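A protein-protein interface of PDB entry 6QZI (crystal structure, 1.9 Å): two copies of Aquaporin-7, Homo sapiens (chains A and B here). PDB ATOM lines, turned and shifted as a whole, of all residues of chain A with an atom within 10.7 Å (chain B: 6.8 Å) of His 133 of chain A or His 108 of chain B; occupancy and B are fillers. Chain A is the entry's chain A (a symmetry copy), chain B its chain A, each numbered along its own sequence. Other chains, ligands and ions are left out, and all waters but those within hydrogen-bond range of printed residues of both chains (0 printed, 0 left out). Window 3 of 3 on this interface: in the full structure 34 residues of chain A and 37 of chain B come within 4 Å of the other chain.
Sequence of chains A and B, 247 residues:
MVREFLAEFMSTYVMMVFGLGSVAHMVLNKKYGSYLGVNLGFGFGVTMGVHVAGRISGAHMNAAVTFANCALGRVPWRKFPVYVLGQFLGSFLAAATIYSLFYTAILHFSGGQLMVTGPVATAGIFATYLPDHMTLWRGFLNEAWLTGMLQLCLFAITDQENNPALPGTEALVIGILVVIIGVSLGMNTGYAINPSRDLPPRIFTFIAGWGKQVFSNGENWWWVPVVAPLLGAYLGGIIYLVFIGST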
ATOM      1  N   TYR A 129      19.021  18.920  24.457  1.00  0.00           N
ATOM      2  CA  TYR A 129      19.322  19.459  25.776  1.00  0.00           C
ATOM      3  C   TYR A 129      20.646  18.884  26.254  1.00  0.00           C
ATOM      4  O   TYR A 129      20.919  17.695  26.069  1.00  0.00           O
ATOM      5  CB  TYR A 129      18.201  19.148  26.776  1.00  0.00           C
ATOM      6  CG  TYR A 129      16.933  19.908  26.472  1.00  0.00           C
ATOM      7  CD1 TYR A 129      16.709  21.168  27.012  1.00  0.00           C
ATOM      8  CD2 TYR A 129      15.977  19.381  25.613  1.00  0.00           C
ATOM      9  CE1 TYR A 129      15.556  21.874  26.721  1.00  0.00           C
ATOM     10  CE2 TYR A 129      14.825  20.079  25.315  1.00  0.00           C
ATOM     11  CZ  TYR A 129      14.618  21.322  25.872  1.00  0.00           C
ATOM     12  OH  TYR A 129      13.470  22.013  25.572  1.00  0.00           O
ATOM     13  N   LEU A 130      21.463  19.738  26.860  1.00  0.00           N
ATOM     14  CA  LEU A 130      22.787  19.327  27.301  1.00  0.00           C
ATOM     15  C   LEU A 130      22.678  18.274  28.398  1.00  0.00           C
ATOM     16  O   LEU A 130      21.986  18.500  29.400  1.00  0.00           O
ATOM     17  CB  LEU A 130      23.572  20.530  27.822  1.00  0.00           C
ATOM     18  CG  LEU A 130      24.561  21.219  26.884  1.00  0.00           C
ATOM     19  CD1 LEU A 130      25.454  22.173  27.666  1.00  0.00           C
ATOM     20  CD2 LEU A 130      25.393  20.199  26.121  1.00  0.00           C
ATOM     21  N   PRO A 131      23.328  17.121  28.251  1.00  0.00           N
ATOM     22  CA  PRO A 131      23.473  16.217  29.395  1.00  0.00           C
ATOM     23  C   PRO A 131      24.258  16.898  30.504  1.00  0.00           C
ATOM     24  O   PRO A 131      25.041  17.823  30.276  1.00  0.00           O
ATOM     25  CB  PRO A 131      24.234  15.017  28.817  1.00  0.00           C
ATOM     26  CG  PRO A 131      24.852  15.517  27.556  1.00  0.00           C
ATOM     27  CD  PRO A 131      23.930  16.570  27.027  1.00  0.00           C
ATOM     28  N   ASP A 132      24.033  16.434  31.731  1.00  0.00           N
ATOM     29  CA  ASP A 132      24.595  17.142  32.871  1.00  0.00           C
ATOM     30  C   ASP A 132      26.103  16.981  32.982  1.00  0.00           C
ATOM     31  O   ASP A 132      26.745  17.772  33.678  1.00  0.00           O
ATOM     32  CB  ASP A 132      23.922  16.687  34.158  1.00  0.00           C
ATOM     33  CG  ASP A 132      23.811  17.801  35.170  1.00  0.00           C
ATOM     34  OD1 ASP A 132      23.000  17.668  36.097  1.00  0.00           O
ATOM     35  OD2 ASP A 132      24.537  18.810  35.043  1.00  0.00           O
ATOM     36  N   HIS A 133      26.688  15.993  32.309  1.00  0.00           N
ATOM     37  CA  HIS A 133      28.139  15.873  32.318  1.00  0.00           C
ATOM     38  C   HIS A 133      28.817  16.894  31.415  1.00  0.00           C
ATOM     39  O   HIS A 133      30.042  17.028  31.472  1.00  0.00           O
ATOM     40  CB  HIS A 133      28.559  14.455  31.913  1.00  0.00           C
ATOM     41  CG  HIS A 133      28.411  14.166  30.451  1.00  0.00           C
ATOM     42  ND1 HIS A 133      27.319  13.505  29.929  1.00  0.00           N
ATOM     43  CD2 HIS A 133      29.227  14.428  29.401  1.00  0.00           C
ATOM     44  CE1 HIS A 133      27.463  13.384  28.621  1.00  0.00           C
ATOM     45  NE2 HIS A 133      28.611  13.935  28.275  1.00  0.00           N
ATOM     46  N   MET A 134      28.058  17.628  30.608  1.00  0.00           N
ATOM     47  CA  MET A 134      28.617  18.505  29.591  1.00  0.00           C
ATOM     48  C   MET A 134      28.661  19.954  30.062  1.00  0.00           C
ATOM     49  O   MET A 134      27.811  20.406  30.833  1.00  0.00           O
ATOM     50  CB  MET A 134      27.798  18.415  28.304  1.00  0.00           C
ATOM     51  CG  MET A 134      28.032  17.143  27.527  1.00  0.00           C
ATOM     52  SD  MET A 134      29.648  17.154  26.743  1.00  0.00           S
ATOM     53  CE  MET A 134      29.460  18.561  25.665  1.00  0.00           C
ATOM     54  N   THR A 135      29.668  20.676  29.584  1.00  0.00           N
ATOM     55  CA  THR A 135      29.742  22.123  29.707  1.00  0.00           C
ATOM     56  C   THR A 135      29.261  22.766  28.411  1.00  0.00           C
ATOM     57  O   THR A 135      29.239  22.136  27.350  1.00  0.00           O
ATOM     58  CB  THR A 135      31.170  22.577  30.022  1.00  0.00           C
ATOM     59  OG1 THR A 135      31.939  22.617  28.813  1.00  0.00           O
ATOM     60  CG2 THR A 135      31.830  21.629  31.015  1.00  0.00           C
ATOM     61  N   LEU A 136      28.869  24.037  28.505  1.00  0.00           N
ATOM     62  CA  LEU A 136      28.375  24.722  27.316  1.00  0.00           C
ATOM     63  C   LEU A 136      29.488  24.923  26.294  1.00  0.00           C
ATOM     64  O   LEU A 136      29.243  24.861  25.084  1.00  0.00           O
ATOM     65  CB  LEU A 136      27.741  26.059  27.695  1.00  0.00           C
ATOM     66  CG  LEU A 136      27.079  26.786  26.522  1.00  0.00           C
ATOM     67  CD1 LEU A 136      25.574  26.578  26.545  1.00  0.00           C
ATOM     68  CD2 LEU A 136      27.418  28.269  26.530  1.00  0.00           C
ATOM     69  N   TRP A 137      30.719  25.152  26.759  1.00  0.00           N
ATOM     70  CA  TRP A 137      31.844  25.292  25.839  1.00  0.00           C
ATOM     71  C   TRP A 137      32.078  24.001  25.063  1.00  0.00           C
ATOM     72  O   TRP A 137      32.216  24.017  23.834  1.00  0.00           O
ATOM     73  CB  TRP A 137      33.108  25.694  26.601  1.00  0.00           C
ATOM     74  CG  TRP A 137      34.363  25.114  26.015  1.00  0.00           C
ATOM     75  CD1 TRP A 137      35.114  24.096  26.527  1.00  0.00           C
ATOM     76  CD2 TRP A 137      35.012  25.519  24.803  1.00  0.00           C
ATOM     77  NE1 TRP A 137      36.190  23.843  25.711  1.00  0.00           N
ATOM     78  CE2 TRP A 137      36.150  24.703  24.645  1.00  0.00           C
ATOM     79  CE3 TRP A 137      34.740  26.493  23.837  1.00  0.00           C
ATOM     80  CZ2 TRP A 137      37.016  24.831  23.561  1.00  0.00           C
ATOM     81  CZ3 TRP A 137      35.601  26.618  22.761  1.00  0.00           C
ATOM     82  CH2 TRP A 137      36.725  25.793  22.632  1.00  0.00           C
ATOM     83  N   ARG A 138      32.135  22.867  25.766  1.00  0.00           N
ATOM     84  CA  ARG A 138      32.346  21.601  25.072  1.00  0.00           C
ATOM     85  C   ARG A 138      31.135  21.214  24.234  1.00  0.00           C
ATOM     86  O   ARG A 138      31.278  20.492  23.242  1.00  0.00           O
ATOM     87  CB  ARG A 138      32.686  20.494  26.069  1.00  0.00           C
ATOM     88  CG  ARG A 138      33.974  19.754  25.724  1.00  0.00           C
ATOM     89  CD  ARG A 138      34.660  19.197  26.957  1.00  0.00           C
ATOM     90  NE  ARG A 138      35.744  20.055  27.423  1.00  0.00           N
ATOM     91  CZ  ARG A 138      36.956  20.092  26.882  1.00  0.00           C
ATOM     92  NH1 ARG A 138      37.249  19.318  25.845  1.00  0.00           N
ATOM     93  NH2 ARG A 138      37.875  20.907  27.381  1.00  0.00           N
ATOM     94  N   GLY A 139      29.942  21.676  24.612  1.00  0.00           N
ATOM     95  CA  GLY A 139      28.786  21.483  23.753  1.00  0.00           C
ATOM     96  C   GLY A 139      28.885  22.288  22.473  1.00  0.00           C
ATOM     97  O   GLY A 139      28.529  21.803  21.394  1.00  0.00           O
ATOM     98  N   ASN A 142      31.377  20.464  20.290  1.00  0.00           N
ATOM     99  CA  ASN A 142      30.804  19.279  19.661  1.00  0.00           C
ATOM    100  C   ASN A 142      29.930  19.655  18.472  1.00  0.00           C
ATOM    101  O   ASN A 142      30.086  19.103  17.377  1.00  0.00           O
ATOM    102  CB  ASN A 142      30.002  18.477  20.688  1.00  0.00           C
ATOM    103  CG  ASN A 142      30.830  17.399  21.360  1.00  0.00           C
ATOM    104  OD1 ASN A 142      30.865  16.256  20.908  1.00  0.00           O
ATOM    105  ND2 ASN A 142      31.505  17.760  22.445  1.00  0.00           N
ATOM    106  N   LEU A 185      28.865  10.120  17.338  1.00  0.00           N
ATOM    107  CA  LEU A 185      29.165  11.424  17.917  1.00  0.00           C
ATOM    108  C   LEU A 185      27.991  12.069  18.646  1.00  0.00           C
ATOM    109  O   LEU A 185      28.121  13.211  19.103  1.00  0.00           O
ATOM    110  CB  LEU A 185      29.665  12.375  16.820  1.00  0.00           C
ATOM    111  CG  LEU A 185      30.892  11.914  16.026  1.00  0.00           C
ATOM    112  CD1 LEU A 185      31.075  12.734  14.757  1.00  0.00           C
ATOM    113  CD2 LEU A 185      32.130  11.992  16.914  1.00  0.00           C
ATOM    114  N   GLY A 186      26.864  11.378  18.791  1.00  0.00           N
ATOM    115  CA  GLY A 186      25.646  12.062  19.182  1.00  0.00           C
ATOM    116  C   GLY A 186      25.314  12.136  20.654  1.00  0.00           C
ATOM    117  O   GLY A 186      24.454  12.937  21.032  1.00  0.00           O
ATOM    118  N   MET A 187      25.953  11.332  21.509  1.00  0.00           N
ATOM    119  CA  MET A 187      25.534  11.274  22.907  1.00  0.00           C
ATOM    120  C   MET A 187      25.898  12.528  23.690  1.00  0.00           C
ATOM    121  O   MET A 187      25.337  12.748  24.767  1.00  0.00           O
ATOM    122  CB  MET A 187      26.142  10.054  23.605  1.00  0.00           C
ATOM    123  CG  MET A 187      27.626  10.190  23.920  1.00  0.00           C
ATOM    124  SD  MET A 187      28.262   8.836  24.930  1.00  0.00           S
ATOM    125  CE  MET A 187      28.552   9.670  26.491  1.00  0.00           C
ATOM    126  N   ASN A 188      26.814  13.353  23.185  1.00  0.00           N
ATOM    127  CA  ASN A 188      27.293  14.472  23.992  1.00  0.00           C
ATOM    128  C   ASN A 188      26.382  15.690  23.904  1.00  0.00           C
ATOM    129  O   ASN A 188      26.295  16.457  24.868  1.00  0.00           O
ATOM    130  CB  ASN A 188      28.717  14.842  23.577  1.00  0.00           C
ATOM    131  CG  ASN A 188      29.715  13.751  23.907  1.00  0.00           C
ATOM    132  OD1 ASN A 188      29.700  13.201  25.006  1.00  0.00           O
ATOM    133  ND2 ASN A 188      30.579  13.423  22.953  1.00  0.00           N
ATOM    134  N   THR A 189      25.709  15.896  22.769  1.00  0.00           N
ATOM    135  CA  THR A 189      24.834  17.052  22.609  1.00  0.00           C
ATOM    136  C   THR A 189      23.513  16.732  21.925  1.00  0.00           C
ATOM    137  O   THR A 189      22.719  17.652  21.705  1.00  0.00           O
ATOM    138  CB  THR A 189      25.533  18.167  21.805  1.00  0.00           C
ATOM    139  OG1 THR A 189      25.882  17.675  20.505  1.00  0.00           O
ATOM    140  CG2 THR A 189      26.783  18.669  22.518  1.00  0.00           C
ATOM    141  N   GLY A 190      23.249  15.476  21.576  1.00  0.00           N
ATOM    142  CA  GLY A 190      22.099  15.174  20.752  1.00  0.00           C
ATOM    143  C   GLY A 190      22.299  15.459  19.283  1.00  0.00           C
ATOM    144  O   GLY A 190      21.316  15.499  18.535  1.00  0.00           O
ATOM    145  N   ASN A 217      17.349  26.185  29.952  1.00  0.00           N
ATOM    146  CA  ASN A 217      17.993  24.971  30.433  1.00  0.00           C
ATOM    147  C   ASN A 217      19.363  24.810  29.785  1.00  0.00           C
ATOM    148  O   ASN A 217      19.607  25.281  28.670  1.00  0.00           O
ATOM    149  CB  ASN A 217      17.113  23.750  30.144  1.00  0.00           C
ATOM    150  CG  ASN A 217      17.678  22.463  30.718  1.00  0.00           C
ATOM    151  OD1 ASN A 217      18.737  21.990  30.305  1.00  0.00           O
ATOM    152  ND2 ASN A 217      16.969  21.891  31.681  1.00  0.00           N
ATOM    153  N   GLY A 218      20.265  24.151  30.506  1.00  0.00           N
ATOM    154  CA  GLY A 218      21.609  23.949  29.992  1.00  0.00           C
ATOM    155  C   GLY A 218      22.374  25.239  29.799  1.00  0.00           C
ATOM    156  O   GLY A 218      23.122  25.373  28.821  1.00  0.00           O
ATOM    157  N   GLU A 219      22.185  26.203  30.703  1.00  0.00           N
ATOM    158  CA  GLU A 219      22.902  27.478  30.673  1.00  0.00           C
ATOM    159  C   GLU A 219      22.640  28.225  29.367  1.00  0.00           C
ATOM    160  O   GLU A 219      23.564  28.647  28.667  1.00  0.00           O
ATOM    161  CB  GLU A 219      24.401  27.263  30.905  1.00  0.00           C
ATOM    162  CG  GLU A 219      24.706  26.370  32.102  1.00  0.00           C
ATOM    163  CD  GLU A 219      26.137  25.864  32.113  1.00  0.00           C
ATOM    164  OE1 GLU A 219      26.332  24.629  32.076  1.00  0.00           O
ATOM    165  OE2 GLU A 219      27.063  26.698  32.166  1.00  0.00           O
ATOM    166  N   TRP A 221      21.256  26.911  26.607  1.00  0.00           N
ATOM    167  CA  TRP A 221      21.794  26.056  25.552  1.00  0.00           C
ATOM    168  C   TRP A 221      21.198  26.368  24.186  1.00  0.00           C
ATOM    169  O   TRP A 221      21.849  26.110  23.170  1.00  0.00           O
ATOM    170  CB  TRP A 221      21.552  24.588  25.910  1.00  0.00           C
ATOM    171  CG  TRP A 221      21.785  23.641  24.777  1.00  0.00           C
ATOM    172  CD1 TRP A 221      20.842  22.927  24.099  1.00  0.00           C
ATOM    173  CD2 TRP A 221      23.047  23.306  24.186  1.00  0.00           C
ATOM    174  NE1 TRP A 221      21.439  22.166  23.120  1.00  0.00           N
ATOM    175  CE2 TRP A 221      22.792  22.381  23.153  1.00  0.00           C
ATOM    176  CE3 TRP A 221      24.366  23.697  24.431  1.00  0.00           C
ATOM    177  CZ2 TRP A 221      23.808  21.842  22.368  1.00  0.00           C
ATOM    178  CZ3 TRP A 221      25.374  23.160  23.651  1.00  0.00           C
ATOM    179  CH2 TRP A 221      25.089  22.244  22.629  1.00  0.00           C
ATOM    180  N   ASN B  29      28.374   4.800  27.721  1.00  0.00           N
ATOM    181  CA  ASN B  29      26.951   4.810  28.064  1.00  0.00           C
ATOM    182  C   ASN B  29      26.245   3.685  27.321  1.00  0.00           C
ATOM    183  O   ASN B  29      26.123   3.734  26.095  1.00  0.00           O
ATOM    184  CB  ASN B  29      26.323   6.161  27.742  1.00  0.00           C
ATOM    185  CG  ASN B  29      25.027   6.388  28.493  1.00  0.00           C
ATOM    186  OD1 ASN B  29      24.246   5.459  28.694  1.00  0.00           O
ATOM    187  ND2 ASN B  29      24.794   7.625  28.919  1.00  0.00           N
ATOM    188  N   LEU B 101      36.289  15.840  22.351  1.00  0.00           N
ATOM    189  CA  LEU B 101      34.833  15.893  22.253  1.00  0.00           C
ATOM    190  C   LEU B 101      34.171  15.152  23.409  1.00  0.00           C
ATOM    191  O   LEU B 101      33.130  15.584  23.915  1.00  0.00           O
ATOM    192  CB  LEU B 101      34.369  15.313  20.914  1.00  0.00           C
ATOM    193  CG  LEU B 101      34.741  16.063  19.633  1.00  0.00           C
ATOM    194  CD1 LEU B 101      34.170  15.358  18.406  1.00  0.00           C
ATOM    195  CD2 LEU B 101      34.273  17.509  19.691  1.00  0.00           C
ATOM    196  N   PHE B 102      34.756  14.032  23.837  1.00  0.00           N
ATOM    197  CA  PHE B 102      34.204  13.207  24.904  1.00  0.00           C
ATOM    198  C   PHE B 102      34.884  13.452  26.249  1.00  0.00           C
ATOM    199  O   PHE B 102      34.719  12.648  27.173  1.00  0.00           O
ATOM    200  CB  PHE B 102      34.314  11.726  24.537  1.00  0.00           C
ATOM    201  CG  PHE B 102      33.395  11.295  23.422  1.00  0.00           C
ATOM    202  CD1 PHE B 102      33.696  11.593  22.100  1.00  0.00           C
ATOM    203  CD2 PHE B 102      32.243  10.574  23.695  1.00  0.00           C
ATOM    204  CE1 PHE B 102      32.857  11.190  21.072  1.00  0.00           C
ATOM    205  CE2 PHE B 102      31.402  10.164  22.670  1.00  0.00           C
ATOM    206  CZ  PHE B 102      31.709  10.473  21.359  1.00  0.00           C
ATOM    207  N   TYR B 103      35.638  14.548  26.379  1.00  0.00           N
ATOM    208  CA  TYR B 103      36.469  14.748  27.565  1.00  0.00           C
ATOM    209  C   TYR B 103      35.653  14.662  28.850  1.00  0.00           C
ATOM    210  O   TYR B 103      36.025  13.945  29.789  1.00  0.00           O
ATOM    211  CB  TYR B 103      37.192  16.092  27.479  1.00  0.00           C
ATOM    212  CG  TYR B 103      38.128  16.342  28.639  1.00  0.00           C
ATOM    213  CD1 TYR B 103      39.328  15.649  28.749  1.00  0.00           C
ATOM    214  CD2 TYR B 103      37.810  17.264  29.629  1.00  0.00           C
ATOM    215  CE1 TYR B 103      40.186  15.872  29.811  1.00  0.00           C
ATOM    216  CE2 TYR B 103      38.664  17.492  30.694  1.00  0.00           C
ATOM    217  CZ  TYR B 103      39.848  16.793  30.779  1.00  0.00           C
ATOM    218  OH  TYR B 103      40.698  17.018  31.837  1.00  0.00           O
ATOM    219  N   THR B 104      34.532  15.381  28.914  1.00  0.00           N
ATOM    220  CA  THR B 104      33.752  15.383  30.146  1.00  0.00           C
ATOM    221  C   THR B 104      33.051  14.049  30.374  1.00  0.00           C
ATOM    222  O   THR B 104      32.888  13.630  31.525  1.00  0.00           O
ATOM    223  CB  THR B 104      32.738  16.526  30.135  1.00  0.00           C
ATOM    224  OG1 THR B 104      31.851  16.379  29.022  1.00  0.00           O
ATOM    225  CG2 THR B 104      33.447  17.867  30.046  1.00  0.00           C
ATOM    226  N   ALA B 105      32.638  13.368  29.302  1.00  0.00           N
ATOM    227  CA  ALA B 105      32.069  12.034  29.462  1.00  0.00           C
ATOM    228  C   ALA B 105      33.106  11.061  30.007  1.00  0.00           C
ATOM    229  O   ALA B 105      32.799  10.237  30.875  1.00  0.00           O
ATOM    230  CB  ALA B 105      31.511  11.532  28.130  1.00  0.00           C
ATOM    231  N   ILE B 106      34.342  11.143  29.508  1.00  0.00           N
ATOM    232  CA  ILE B 106      35.410  10.281  30.008  1.00  0.00           C
ATOM    233  C   ILE B 106      35.703  10.594  31.470  1.00  0.00           C
ATOM    234  O   ILE B 106      35.941   9.689  32.281  1.00  0.00           O
ATOM    235  CB  ILE B 106      36.667  10.432  29.130  1.00  0.00           C
ATOM    236  CG1 ILE B 106      36.411   9.867  27.731  1.00  0.00           C
ATOM    237  CG2 ILE B 106      37.867   9.751  29.780  1.00  0.00           C
ATOM    238  CD1 ILE B 106      37.387  10.357  26.684  1.00  0.00           C
ATOM    239  N   LEU B 107      35.670  11.876  31.835  1.00  0.00           N
ATOM    240  CA  LEU B 107      35.971  12.260  33.210  1.00  0.00           C
ATOM    241  C   LEU B 107      34.819  11.923  34.149  1.00  0.00           C
ATOM    242  O   LEU B 107      35.045  11.483  35.282  1.00  0.00           O
ATOM    243  CB  LEU B 107      36.309  13.749  33.268  1.00  0.00           C
ATOM    244  CG  LEU B 107      37.807  14.055  33.345  1.00  0.00           C
ATOM    245  CD1 LEU B 107      38.506  13.675  32.048  1.00  0.00           C
ATOM    246  CD2 LEU B 107      38.044  15.519  33.682  1.00  0.00           C
ATOM    247  N   HIS B 108      33.576  12.124  33.702  1.00  0.00           N
ATOM    248  CA  HIS B 108      32.428  11.754  34.526  1.00  0.00           C
ATOM    249  C   HIS B 108      32.341  10.244  34.700  1.00  0.00           C
ATOM    250  O   HIS B 108      31.976   9.754  35.776  1.00  0.00           O
ATOM    251  CB  HIS B 108      31.141  12.296  33.905  1.00  0.00           C
ATOM    252  CG  HIS B 108      29.893  11.772  34.543  1.00  0.00           C
ATOM    253  ND1 HIS B 108      29.559  12.033  35.855  1.00  0.00           N
ATOM    254  CD2 HIS B 108      28.897  10.997  34.049  1.00  0.00           C
ATOM    255  CE1 HIS B 108      28.412  11.444  36.141  1.00  0.00           C
ATOM    256  NE2 HIS B 108      27.989  10.809  35.063  1.00  0.00           N
ATOM    257  N   PHE B 109      32.675   9.493  33.651  1.00  0.00           N
ATOM    258  CA  PHE B 109      32.595   8.038  33.705  1.00  0.00           C
ATOM    259  C   PHE B 109      33.636   7.462  34.657  1.00  0.00           C
ATOM    260  O   PHE B 109      33.327   6.597  35.485  1.00  0.00           O
ATOM    261  CB  PHE B 109      32.775   7.472  32.296  1.00  0.00           C
ATOM    262  CG  PHE B 109      32.829   5.974  32.233  1.00  0.00           C
ATOM    263  CD1 PHE B 109      31.671   5.221  32.313  1.00  0.00           C
ATOM    264  CD2 PHE B 109      34.038   5.320  32.065  1.00  0.00           C
ATOM    265  CE1 PHE B 109      31.718   3.843  32.242  1.00  0.00           C
ATOM    266  CE2 PHE B 109      34.090   3.943  31.991  1.00  0.00           C
ATOM    267  CZ  PHE B 109      32.929   3.203  32.083  1.00  0.00           C
ATOM    268  N   SER B 110      34.873   7.936  34.559  1.00  0.00           N
ATOM    269  CA  SER B 110      35.986   7.367  35.303  1.00  0.00           C
ATOM    270  C   SER B 110      36.220   8.043  36.647  1.00  0.00           C
ATOM    271  O   SER B 110      37.141   7.647  37.369  1.00  0.00           O
ATOM    272  CB  SER B 110      37.264   7.445  34.464  1.00  0.00           C
ATOM    273  OG  SER B 110      37.621   8.791  34.200  1.00  0.00           O
ATOM    274  N   GLY B 111      35.414   9.040  37.005  1.00  0.00           N
ATOM    275  CA  GLY B 111      35.679   9.794  38.214  1.00  0.00           C
ATOM    276  C   GLY B 111      36.927  10.642  38.152  1.00  0.00           C
ATOM    277  O   GLY B 111      37.408  11.096  39.192  1.00  0.00           O
ATOM    278  N   GLY B 112      37.466  10.871  36.955  1.00  0.00           N
ATOM    279  CA  GLY B 112      38.689  11.623  36.777  1.00  0.00           C
ATOM    280  C   GLY B 112      39.935  10.785  36.605  1.00  0.00           C
ATOM    281  O   GLY B 112      41.020  11.350  36.419  1.00  0.00           O
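ND2 of Asn 142 of chain A lies within hydrogen-bond range of O of Leu 101 of chain B. The backbone carbonyl oxygen (O) of Leu 101 of chain B lies within hydrogen-bond range of the side-chain amide nitrogen (ND2) of Asn 188 of chain A, at 3.5 Å. The backbone carbonyl oxygen (O) of His 133 of chain A lies close to the side-chain hydroxyl (OG1) of Thr 104 of chain B, at 3.1 Å. The side-chain hydroxyl (OG1) of Thr 104 of chain B sits at hydrogen-bond distance from the side-chain sulfur (SD) of Met 134 of chain A (3.3 Å).
A ring nitrogen (NE2) of His 133 of chain A lies close to the side-chain sulfur (SD) of Met 134 of chain A (3.7 Å). N of Arg 138 of chain A lies within hydrogen-bond range of OG1 of Thr 135 of chain A. ND2 of Asn 142 of chain A sits at hydrogen-bond distance from O of Arg 138 of chain A.
His 133 of chain A touches Ala 105 of chain B. CB of His 133 of chain A touches CB of His 108 of chain B (3.9 Å). Arg 138 of chain A touches Tyr 103 of chain B (NH1 to CB, 3.6 Å). CD of Arg 138 of chain A touches CG2 of Thr 104 of chain B (3.6 Å). Phe 102 of chain B touches Met 187 of chain A (CE2 to CG, 3.98 Å). CE of Met 187 of chain A touches CB of Ala 105 of chain B (3.9 Å). Asn 188 of chain A touches Phe 102 of chain B. Ala 105 of chain B touches Asn 188 of chain A (CB to OD1, 3.98 Å).
His 133 of chain A touches just these residues of chain B: Thr 104, Ala 105 and His 108. Of chain A, only His 133 (3.9 Å) comes within 4 Å of His 108 of chain B. Thr 104 of chain B touches three residues of chain A. No residue of chain A comes within 4 Å of Leu 107 of chain B. No residue of chain A comes within 4 Å of Ser 110 of chain B. No residue of chain A comes within 4 Å of Gly 111 of chain B. Printed residues of chain B within 4 Å of Asn 142 of chain A: Leu 101 (3.1 Å). Printed residues of chain B within 4 Å of Met 134 of chain A: Thr 104 (3.3 Å). Printed residues of chain B within 4 Å of Asn 188 of chain A: Leu 101 (3.5 Å), Phe 102 (3.4 Å) and Ala 105 (3.98 Å). Printed residues of chain A within 4 Å of Phe 102 of chain B: Met 187 (3.98 Å) and Asn 188 (3.4 Å). Of the printed residues of chain B, Met 187 of chain A touches Phe 102 and Ala 105. The nearest residue of chain A that does not touch His 108 of chain B is Asp 132 of chain A (6.6 Å). The nearest printed residue of chain B that does not touch Met 187 of chain A is Asn 29 of chain B (4.3 Å).
Hydrophobic or aromatic side chains of chain B within 4 Å of the printed part of chain A: Leu 101, Phe 102, Tyr 103, Ala 105 and His 108. Printed residues of chain A that touch a printed residue of chain B: His 133, Met 134, Arg 138, Asn 142, Met 187 and Asn 188. Hydrophobic or aromatic side chains of chain A within 4 Å of the printed part of chain B: His 133, Met 134 and Met 187. Along chain A the printed residues that touch a printed residue of chain B span positions 133 to 188. Among the printed residues, no Asp or Glu carboxylate lies within 4 Å of a Lys or Arg side-chain nitrogen of the other chain.
No position is printed for both chains.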
